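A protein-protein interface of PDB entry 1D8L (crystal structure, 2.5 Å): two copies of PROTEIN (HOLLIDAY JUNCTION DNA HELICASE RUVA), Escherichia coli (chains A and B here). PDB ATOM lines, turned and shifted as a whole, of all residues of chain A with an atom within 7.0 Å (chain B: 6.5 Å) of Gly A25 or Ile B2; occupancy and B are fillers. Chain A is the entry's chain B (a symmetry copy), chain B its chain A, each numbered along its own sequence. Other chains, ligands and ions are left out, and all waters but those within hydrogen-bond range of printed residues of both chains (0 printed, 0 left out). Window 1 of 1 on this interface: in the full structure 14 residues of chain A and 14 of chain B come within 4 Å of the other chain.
Gly A25 touches just these residues of chain B: Met B1, Ile B2, Gly B3 and Arg B4. Ile B2 touches one residue of chain A. Printed residues of chain B within 4 Å of Glu A20: Arg B4 and Arg B6. Printed residues of chain B within 4 Å of Ile A10: Arg B4 (3.5 Å). Ile A19 touches none of the printed residues of chain B. Val A17 touches none of the printed residues of chain B.
Of the 12 printed residues of chain B, 8 touch a printed residue of chain A. Of the 14 printed residues of chain A, 10 touch a printed residue of chain B. Printed residues of chain A that touch a printed residue of chain B: Ile A10, Glu A20, Gly A22, Gly A23, Val A24, Gly A25, Tyr A26, Glu A27, Gln A58 and Leu A60. Hydrophobic or aromatic side chains of chain A within 4 Å of the printed part of chain B: Ile A10 and Leu A60.
Positions printed for both chains: 26 and 60.
Among the printed residues, pairs that only touch across the chains: Tyr A26 with Met B1 (3.3 Å), Gly A23 with Leu B5 (3.5 Å), Ile A10 with Arg B4 (3.5 Å), Gln A58 with Phe B51 (3.6 Å), Val A24 with Arg B4 (3.6 Å), Gly A25 with Ile B2 (3.6 Å), Glu A27 with Gly B3 (3.6 Å), Gly A23 with Arg B4 (3.7 Å), Gly A22 with Arg B6 (3.7 Å), Leu A60 with Met B1 (3.8 Å) and Gly A25 with Met B1 (3.9 Å).
The side-chain carboxylate of Glu A27 is in salt-bridge range of the guanidinium group of Arg B69 (3.8 Å). The backbone carbonyl oxygen of Gly A25 is in hydrogen-bond range of the backbone NH of Gly B3 (2.8 Å). The side-chain carboxylate (OE1) of Glu A20 lies within salt-bridge range of the guanidinium group (NH2) of Arg B6, at 2.8 Å. N of Glu A27 lies within hydrogen-bond range of O of Met B1. N of Met B1 lies within hydrogen-bond range of O of Gln A58 (3.3 Å). The backbone carbonyl oxygen of Gly A23 is in hydrogen-bond range of the backbone NH of Arg B6 (2.9 Å). The backbone carbonyl oxygen (O) of Arg B4 is in hydrogen-bond range of the backbone NH (N) of Gly A25 (2.6 Å). OE2 of Glu A20 is in salt-bridge range of NH2 of Arg B4, 2.7 Å away.
The backbone carbonyl oxygen (O) of Ile B2 sits at hydrogen-bond distance from the side-chain hydroxyl (OG1) of Thr B49, 3.0 Å away. The guanidinium group (NH1) of Arg B69 sits close to the backbone carbonyl oxygen (O) of Thr B49 (3.3 Å). O of Ile A19 sits at hydrogen-bond distance from N of Tyr A26 (2.9 Å). The backbone NH (N) of Ile A10 lies within hydrogen-bond range of the backbone carbonyl oxygen (O) of Leu A18 (2.6 Å). N of Thr B49 sits at hydrogen-bond distance from O of Gly B3 (3.1 Å). The backbone carbonyl oxygen of Gly B3 lies within hydrogen-bond range of the guanidinium group of Arg B69.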
ATOM      1  N   ILE A  10     -30.037  18.936 -11.054  1.00  0.00           N
ATOM      2  CA  ILE A  10     -28.846  19.650 -11.510  1.00  0.00           C
ATOM      3  C   ILE A  10     -29.221  20.563 -12.667  1.00  0.00           C
ATOM      4  O   ILE A  10     -28.869  21.737 -12.643  1.00  0.00           O
ATOM      5  CB  ILE A  10     -27.728  18.691 -11.923  1.00  0.00           C
ATOM      6  CG1 ILE A  10     -27.270  17.851 -10.731  1.00  0.00           C
ATOM      7  CG2 ILE A  10     -26.554  19.445 -12.542  1.00  0.00           C
ATOM      8  CD1 ILE A  10     -26.700  18.647  -9.580  1.00  0.00           C
ATOM      9  N   VAL A  17     -34.007  15.475 -17.545  1.00  0.00           N
ATOM     10  CA  VAL A  17     -33.754  16.000 -16.225  1.00  0.00           C
ATOM     11  C   VAL A  17     -32.448  15.348 -15.742  1.00  0.00           C
ATOM     12  O   VAL A  17     -32.292  14.145 -15.918  1.00  0.00           O
ATOM     13  CB  VAL A  17     -34.778  15.757 -15.109  1.00  0.00           C
ATOM     14  CG1 VAL A  17     -34.520  16.741 -13.960  1.00  0.00           C
ATOM     15  CG2 VAL A  17     -36.204  15.918 -15.584  1.00  0.00           C
ATOM     16  N   LEU A  18     -31.569  16.148 -15.172  1.00  0.00           N
ATOM     17  CA  LEU A  18     -30.311  15.635 -14.636  1.00  0.00           C
ATOM     18  C   LEU A  18     -30.427  15.724 -13.111  1.00  0.00           C
ATOM     19  O   LEU A  18     -30.552  16.816 -12.539  1.00  0.00           O
ATOM     20  CB  LEU A  18     -29.121  16.367 -15.204  1.00  0.00           C
ATOM     21  CG  LEU A  18     -27.711  15.921 -14.819  1.00  0.00           C
ATOM     22  CD1 LEU A  18     -27.367  14.543 -15.368  1.00  0.00           C
ATOM     23  CD2 LEU A  18     -26.686  16.925 -15.344  1.00  0.00           C
ATOM     24  N   ILE A  19     -30.511  14.555 -12.478  1.00  0.00           N
ATOM     25  CA  ILE A  19     -30.704  14.533 -11.028  1.00  0.00           C
ATOM     26  C   ILE A  19     -29.495  13.826 -10.435  1.00  0.00           C
ATOM     27  O   ILE A  19     -29.106  12.765 -10.906  1.00  0.00           O
ATOM     28  CB  ILE A  19     -32.051  13.924 -10.620  1.00  0.00           C
ATOM     29  CG1 ILE A  19     -32.182  13.780  -9.104  1.00  0.00           C
ATOM     30  CG2 ILE A  19     -32.248  12.558 -11.261  1.00  0.00           C
ATOM     31  CD1 ILE A  19     -33.606  13.653  -8.603  1.00  0.00           C
ATOM     32  N   GLU A  20     -28.890  14.485  -9.449  1.00  0.00           N
ATOM     33  CA  GLU A  20     -27.675  13.986  -8.834  1.00  0.00           C
ATOM     34  C   GLU A  20     -28.022  13.257  -7.545  1.00  0.00           C
ATOM     35  O   GLU A  20     -28.692  13.786  -6.665  1.00  0.00           O
ATOM     36  CB  GLU A  20     -26.657  15.110  -8.623  1.00  0.00           C
ATOM     37  CG  GLU A  20     -25.235  14.629  -8.484  1.00  0.00           C
ATOM     38  CD  GLU A  20     -24.235  15.610  -7.915  1.00  0.00           C
ATOM     39  OE1 GLU A  20     -24.468  16.149  -6.809  1.00  0.00           O
ATOM     40  OE2 GLU A  20     -23.185  15.848  -8.560  1.00  0.00           O
ATOM     41  N   VAL A  21     -27.644  11.993  -7.495  1.00  0.00           N
ATOM     42  CA  VAL A  21     -27.884  11.098  -6.379  1.00  0.00           C
ATOM     43  C   VAL A  21     -26.501  10.624  -5.931  1.00  0.00           C
ATOM     44  O   VAL A  21     -25.892   9.833  -6.648  1.00  0.00           O
ATOM     45  CB  VAL A  21     -28.740   9.885  -6.751  1.00  0.00           C
ATOM     46  CG1 VAL A  21     -28.982   9.039  -5.507  1.00  0.00           C
ATOM     47  CG2 VAL A  21     -30.074  10.248  -7.398  1.00  0.00           C
ATOM     48  N   GLY A  22     -26.020  11.161  -4.820  1.00  0.00           N
ATOM     49  CA  GLY A  22     -24.639  10.856  -4.399  1.00  0.00           C
ATOM     50  C   GLY A  22     -23.809  11.796  -5.295  1.00  0.00           C
ATOM     51  O   GLY A  22     -24.040  13.007  -5.253  1.00  0.00           O
ATOM     52  N   GLY A  23     -22.944  11.256  -6.135  1.00  0.00           N
ATOM     53  CA  GLY A  23     -22.223  12.108  -7.075  1.00  0.00           C
ATOM     54  C   GLY A  23     -22.532  11.626  -8.505  1.00  0.00           C
ATOM     55  O   GLY A  23     -21.872  12.021  -9.465  1.00  0.00           O
ATOM     56  N   VAL A  24     -23.545  10.772  -8.624  1.00  0.00           N
ATOM     57  CA  VAL A  24     -23.902  10.230  -9.936  1.00  0.00           C
ATOM     58  C   VAL A  24     -25.047  11.007 -10.542  1.00  0.00           C
ATOM     59  O   VAL A  24     -26.137  10.943 -10.002  1.00  0.00           O
ATOM     60  CB  VAL A  24     -24.256   8.741  -9.840  1.00  0.00           C
ATOM     61  CG1 VAL A  24     -24.735   8.175 -11.162  1.00  0.00           C
ATOM     62  CG2 VAL A  24     -23.044   7.960  -9.338  1.00  0.00           C
ATOM     63  N   GLY A  25     -24.795  11.729 -11.624  1.00  0.00           N
ATOM     64  CA  GLY A  25     -25.861  12.482 -12.291  1.00  0.00           C
ATOM     65  C   GLY A  25     -26.584  11.542 -13.253  1.00  0.00           C
ATOM     66  O   GLY A  25     -25.989  11.094 -14.227  1.00  0.00           O
ATOM     67  N   TYR A  26     -27.811  11.192 -12.954  1.00  0.00           N
ATOM     68  CA  TYR A  26     -28.653  10.300 -13.735  1.00  0.00           C
ATOM     69  C   TYR A  26     -29.534  11.063 -14.720  1.00  0.00           C
ATOM     70  O   TYR A  26     -30.211  12.020 -14.329  1.00  0.00           O
ATOM     71  CB  TYR A  26     -29.603   9.514 -12.807  1.00  0.00           C
ATOM     72  CG  TYR A  26     -28.964   8.366 -12.068  1.00  0.00           C
ATOM     73  CD1 TYR A  26     -28.575   7.204 -12.739  1.00  0.00           C
ATOM     74  CD2 TYR A  26     -28.717   8.440 -10.703  1.00  0.00           C
ATOM     75  CE1 TYR A  26     -27.977   6.156 -12.065  1.00  0.00           C
ATOM     76  CE2 TYR A  26     -28.107   7.407 -10.012  1.00  0.00           C
ATOM     77  CZ  TYR A  26     -27.753   6.265 -10.706  1.00  0.00           C
ATOM     78  OH  TYR A  26     -27.157   5.227 -10.026  1.00  0.00           O
ATOM     79  N   GLU A  27     -29.552  10.629 -15.980  1.00  0.00           N
ATOM     80  CA  GLU A  27     -30.403  11.267 -16.983  1.00  0.00           C
ATOM     81  C   GLU A  27     -31.784  10.616 -16.953  1.00  0.00           C
ATOM     82  O   GLU A  27     -31.875   9.406 -17.061  1.00  0.00           O
ATOM     83  CB  GLU A  27     -29.859  11.150 -18.392  1.00  0.00           C
ATOM     84  CG  GLU A  27     -28.387  11.463 -18.540  1.00  0.00           C
ATOM     85  CD  GLU A  27     -28.031  11.777 -19.975  1.00  0.00           C
ATOM     86  OE1 GLU A  27     -28.640  11.161 -20.872  1.00  0.00           O
ATOM     87  OE2 GLU A  27     -27.168  12.644 -20.192  1.00  0.00           O
ATOM     88  N   GLN A  58     -29.243   1.832 -21.914  1.00  0.00           N
ATOM     89  CA  GLN A  58     -29.831   1.767 -20.581  1.00  0.00           C
ATOM     90  C   GLN A  58     -30.541   3.101 -20.374  1.00  0.00           C
ATOM     91  O   GLN A  58     -29.905   4.150 -20.377  1.00  0.00           O
ATOM     92  CB  GLN A  58     -28.849   1.466 -19.470  1.00  0.00           C
ATOM     93  CG  GLN A  58     -28.517  -0.008 -19.348  1.00  0.00           C
ATOM     94  CD  GLN A  58     -27.550  -0.375 -18.253  1.00  0.00           C
ATOM     95  OE1 GLN A  58     -26.838  -1.379 -18.370  1.00  0.00           O
ATOM     96  NE2 GLN A  58     -27.509   0.410 -17.184  1.00  0.00           N
ATOM     97  N   LEU A  60     -33.722   5.564 -18.473  1.00  0.00           N
ATOM     98  CA  LEU A  60     -34.566   5.878 -17.326  1.00  0.00           C
ATOM     99  C   LEU A  60     -35.728   6.767 -17.774  1.00  0.00           C
ATOM    100  O   LEU A  60     -35.495   7.782 -18.425  1.00  0.00           O
ATOM    101  CB  LEU A  60     -33.784   6.575 -16.235  1.00  0.00           C
ATOM    102  CG  LEU A  60     -33.477   5.938 -14.898  1.00  0.00           C
ATOM    103  CD1 LEU A  60     -33.649   4.435 -14.845  1.00  0.00           C
ATOM    104  CD2 LEU A  60     -32.053   6.311 -14.470  1.00  0.00           C
ATOM    105  N   MET B   1     -27.663   6.290 -19.180  1.00  0.00           N
ATOM    106  CA  MET B   1     -28.469   6.975 -18.123  1.00  0.00           C
ATOM    107  C   MET B   1     -27.584   7.771 -17.174  1.00  0.00           C
ATOM    108  O   MET B   1     -28.026   8.736 -16.569  1.00  0.00           O
ATOM    109  CB  MET B   1     -29.353   5.974 -17.396  1.00  0.00           C
ATOM    110  CG  MET B   1     -28.679   4.645 -17.101  1.00  0.00           C
ATOM    111  SD  MET B   1     -29.359   3.869 -15.625  1.00  0.00           S
ATOM    112  CE  MET B   1     -27.926   3.034 -14.963  1.00  0.00           C
ATOM    113  N   ILE B   2     -26.304   7.445 -17.081  1.00  0.00           N
ATOM    114  CA  ILE B   2     -25.346   8.218 -16.325  1.00  0.00           C
ATOM    115  C   ILE B   2     -24.848   9.390 -17.175  1.00  0.00           C
ATOM    116  O   ILE B   2     -24.089   9.141 -18.117  1.00  0.00           O
ATOM    117  CB  ILE B   2     -24.146   7.370 -15.877  1.00  0.00           C
ATOM    118  CG1 ILE B   2     -24.641   6.140 -15.120  1.00  0.00           C
ATOM    119  CG2 ILE B   2     -23.232   8.232 -15.003  1.00  0.00           C
ATOM    120  CD1 ILE B   2     -23.574   5.320 -14.437  1.00  0.00           C
ATOM    121  N   GLY B   3     -25.228  10.625 -16.842  1.00  0.00           N
ATOM    122  CA  GLY B   3     -24.815  11.786 -17.610  1.00  0.00           C
ATOM    123  C   GLY B   3     -23.764  12.667 -16.951  1.00  0.00           C
ATOM    124  O   GLY B   3     -23.148  13.518 -17.604  1.00  0.00           O
ATOM    125  N   ARG B   4     -23.488  12.458 -15.668  1.00  0.00           N
ATOM    126  CA  ARG B   4     -22.476  13.229 -14.954  1.00  0.00           C
ATOM    127  C   ARG B   4     -21.936  12.468 -13.745  1.00  0.00           C
ATOM    128  O   ARG B   4     -22.616  11.701 -13.070  1.00  0.00           O
ATOM    129  CB  ARG B   4     -23.013  14.586 -14.500  1.00  0.00           C
ATOM    130  CG  ARG B   4     -22.020  15.735 -14.498  1.00  0.00           C
ATOM    131  CD  ARG B   4     -22.627  17.022 -13.934  1.00  0.00           C
ATOM    132  NE  ARG B   4     -22.659  17.012 -12.478  1.00  0.00           N
ATOM    133  CZ  ARG B   4     -22.864  18.029 -11.651  1.00  0.00           C
ATOM    134  NH1 ARG B   4     -23.075  19.259 -12.089  1.00  0.00           N
ATOM    135  NH2 ARG B   4     -22.865  17.829 -10.340  1.00  0.00           N
ATOM    136  N   LEU B   5     -20.650  12.697 -13.479  1.00  0.00           N
ATOM    137  CA  LEU B   5     -19.963  12.109 -12.348  1.00  0.00           C
ATOM    138  C   LEU B   5     -19.235  13.222 -11.586  1.00  0.00           C
ATOM    139  O   LEU B   5     -18.544  14.053 -12.171  1.00  0.00           O
ATOM    140  CB  LEU B   5     -18.957  11.047 -12.775  1.00  0.00           C
ATOM    141  CG  LEU B   5     -19.442   9.647 -13.146  1.00  0.00           C
ATOM    142  CD1 LEU B   5     -18.247   8.749 -13.439  1.00  0.00           C
ATOM    143  CD2 LEU B   5     -20.305   9.031 -12.059  1.00  0.00           C
ATOM    144  N   ARG B   6     -19.414  13.244 -10.276  1.00  0.00           N
ATOM    145  CA  ARG B   6     -18.742  14.188  -9.410  1.00  0.00           C
ATOM    146  C   ARG B   6     -18.087  13.401  -8.272  1.00  0.00           C
ATOM    147  O   ARG B   6     -18.795  12.820  -7.449  1.00  0.00           O
ATOM    148  CB  ARG B   6     -19.676  15.252  -8.843  1.00  0.00           C
ATOM    149  CG  ARG B   6     -18.941  16.204  -7.895  1.00  0.00           C
ATOM    150  CD  ARG B   6     -19.809  17.399  -7.540  1.00  0.00           C
ATOM    151  NE  ARG B   6     -21.022  16.977  -6.845  1.00  0.00           N
ATOM    152  CZ  ARG B   6     -21.117  16.637  -5.563  1.00  0.00           C
ATOM    153  NH1 ARG B   6     -20.049  16.665  -4.777  1.00  0.00           N
ATOM    154  NH2 ARG B   6     -22.302  16.277  -5.094  1.00  0.00           N
ATOM    155  N   TYR B  26     -14.788   4.631 -10.679  1.00  0.00           N
ATOM    156  CA  TYR B  26     -15.204   4.553 -12.066  1.00  0.00           C
ATOM    157  C   TYR B  26     -14.122   4.859 -13.092  1.00  0.00           C
ATOM    158  O   TYR B  26     -13.479   5.917 -13.003  1.00  0.00           O
ATOM    159  CB  TYR B  26     -16.305   5.607 -12.299  1.00  0.00           C
ATOM    160  CG  TYR B  26     -17.671   5.186 -11.810  1.00  0.00           C
ATOM    161  CD1 TYR B  26     -18.388   4.200 -12.472  1.00  0.00           C
ATOM    162  CD2 TYR B  26     -18.236   5.791 -10.688  1.00  0.00           C
ATOM    163  CE1 TYR B  26     -19.641   3.813 -12.035  1.00  0.00           C
ATOM    164  CE2 TYR B  26     -19.486   5.411 -10.237  1.00  0.00           C
ATOM    165  CZ  TYR B  26     -20.176   4.424 -10.921  1.00  0.00           C
ATOM    166  OH  TYR B  26     -21.419   4.046 -10.472  1.00  0.00           O
ATOM    167  N   THR B  49     -20.432  12.758 -18.858  1.00  0.00           N
ATOM    168  CA  THR B  49     -20.218  11.429 -19.397  1.00  0.00           C
ATOM    169  C   THR B  49     -21.239  10.999 -20.445  1.00  0.00           C
ATOM    170  O   THR B  49     -22.350  11.480 -20.559  1.00  0.00           O
ATOM    171  CB  THR B  49     -20.209  10.402 -18.240  1.00  0.00           C
ATOM    172  OG1 THR B  49     -21.469  10.448 -17.563  1.00  0.00           O
ATOM    173  CG2 THR B  49     -19.115  10.696 -17.219  1.00  0.00           C
ATOM    174  N   HIS B  50     -20.833  10.013 -21.243  1.00  0.00           N
ATOM    175  CA  HIS B  50     -21.673   9.367 -22.240  1.00  0.00           C
ATOM    176  C   HIS B  50     -21.526   7.866 -21.994  1.00  0.00           C
ATOM    177  O   HIS B  50     -20.400   7.387 -22.072  1.00  0.00           O
ATOM    178  CB  HIS B  50     -21.300   9.705 -23.665  1.00  0.00           C
ATOM    179  CG  HIS B  50     -22.145   9.023 -24.698  1.00  0.00           C
ATOM    180  ND1 HIS B  50     -23.468   9.353 -24.898  1.00  0.00           N
ATOM    181  CD2 HIS B  50     -21.854   8.029 -25.573  1.00  0.00           C
ATOM    182  CE1 HIS B  50     -23.956   8.593 -25.866  1.00  0.00           C
ATOM    183  NE2 HIS B  50     -22.995   7.787 -26.292  1.00  0.00           N
ATOM    184  N   PHE B  51     -22.608   7.194 -21.633  1.00  0.00           N
ATOM    185  CA  PHE B  51     -22.557   5.768 -21.337  1.00  0.00           C
ATOM    186  C   PHE B  51     -22.756   4.892 -22.575  1.00  0.00           C
ATOM    187  O   PHE B  51     -23.820   4.916 -23.202  1.00  0.00           O
ATOM    188  CB  PHE B  51     -23.624   5.479 -20.288  1.00  0.00           C
ATOM    189  CG  PHE B  51     -23.612   4.166 -19.570  1.00  0.00           C
ATOM    190  CD1 PHE B  51     -22.458   3.441 -19.333  1.00  0.00           C
ATOM    191  CD2 PHE B  51     -24.815   3.650 -19.083  1.00  0.00           C
ATOM    192  CE1 PHE B  51     -22.501   2.244 -18.656  1.00  0.00           C
ATOM    193  CE2 PHE B  51     -24.858   2.445 -18.395  1.00  0.00           C
ATOM    194  CZ  PHE B  51     -23.697   1.736 -18.176  1.00  0.00           C
ATOM    195  N   LEU B  60     -17.592   4.238 -20.264  1.00  0.00           N
ATOM    196  CA  LEU B  60     -17.857   5.635 -19.955  1.00  0.00           C
ATOM    197  C   LEU B  60     -16.830   6.533 -20.651  1.00  0.00           C
ATOM    198  O   LEU B  60     -15.617   6.377 -20.570  1.00  0.00           O
ATOM    199  CB  LEU B  60     -17.848   5.802 -18.456  1.00  0.00           C
ATOM    200  CG  LEU B  60     -18.998   6.324 -17.639  1.00  0.00           C
ATOM    201  CD1 LEU B  60     -20.381   6.080 -18.208  1.00  0.00           C
ATOM    202  CD2 LEU B  60     -18.891   5.736 -16.223  1.00  0.00           C
ATOM    203  N   ARG B  69     -19.191  16.895 -25.334  1.00  0.00           N
ATOM    204  CA  ARG B  69     -19.938  15.648 -25.248  1.00  0.00           C
ATOM    205  C   ARG B  69     -20.893  15.557 -26.437  1.00  0.00           C
ATOM    206  O   ARG B  69     -21.045  14.524 -27.089  1.00  0.00           O
ATOM    207  CB  ARG B  69     -20.696  15.520 -23.931  1.00  0.00           C
ATOM    208  CG  ARG B  69     -21.508  14.230 -23.875  1.00  0.00           C
ATOM    209  CD  ARG B  69     -22.220  14.101 -22.543  1.00  0.00           C
ATOM    210  NE  ARG B  69     -23.203  15.175 -22.398  1.00  0.00           N
ATOM    211  CZ  ARG B  69     -23.974  15.286 -21.325  1.00  0.00           C
ATOM    212  NH1 ARG B  69     -23.846  14.404 -20.346  1.00  0.00           N
ATOM    213  NH2 ARG B  69     -24.843  16.274 -21.256  1.00  0.00           N
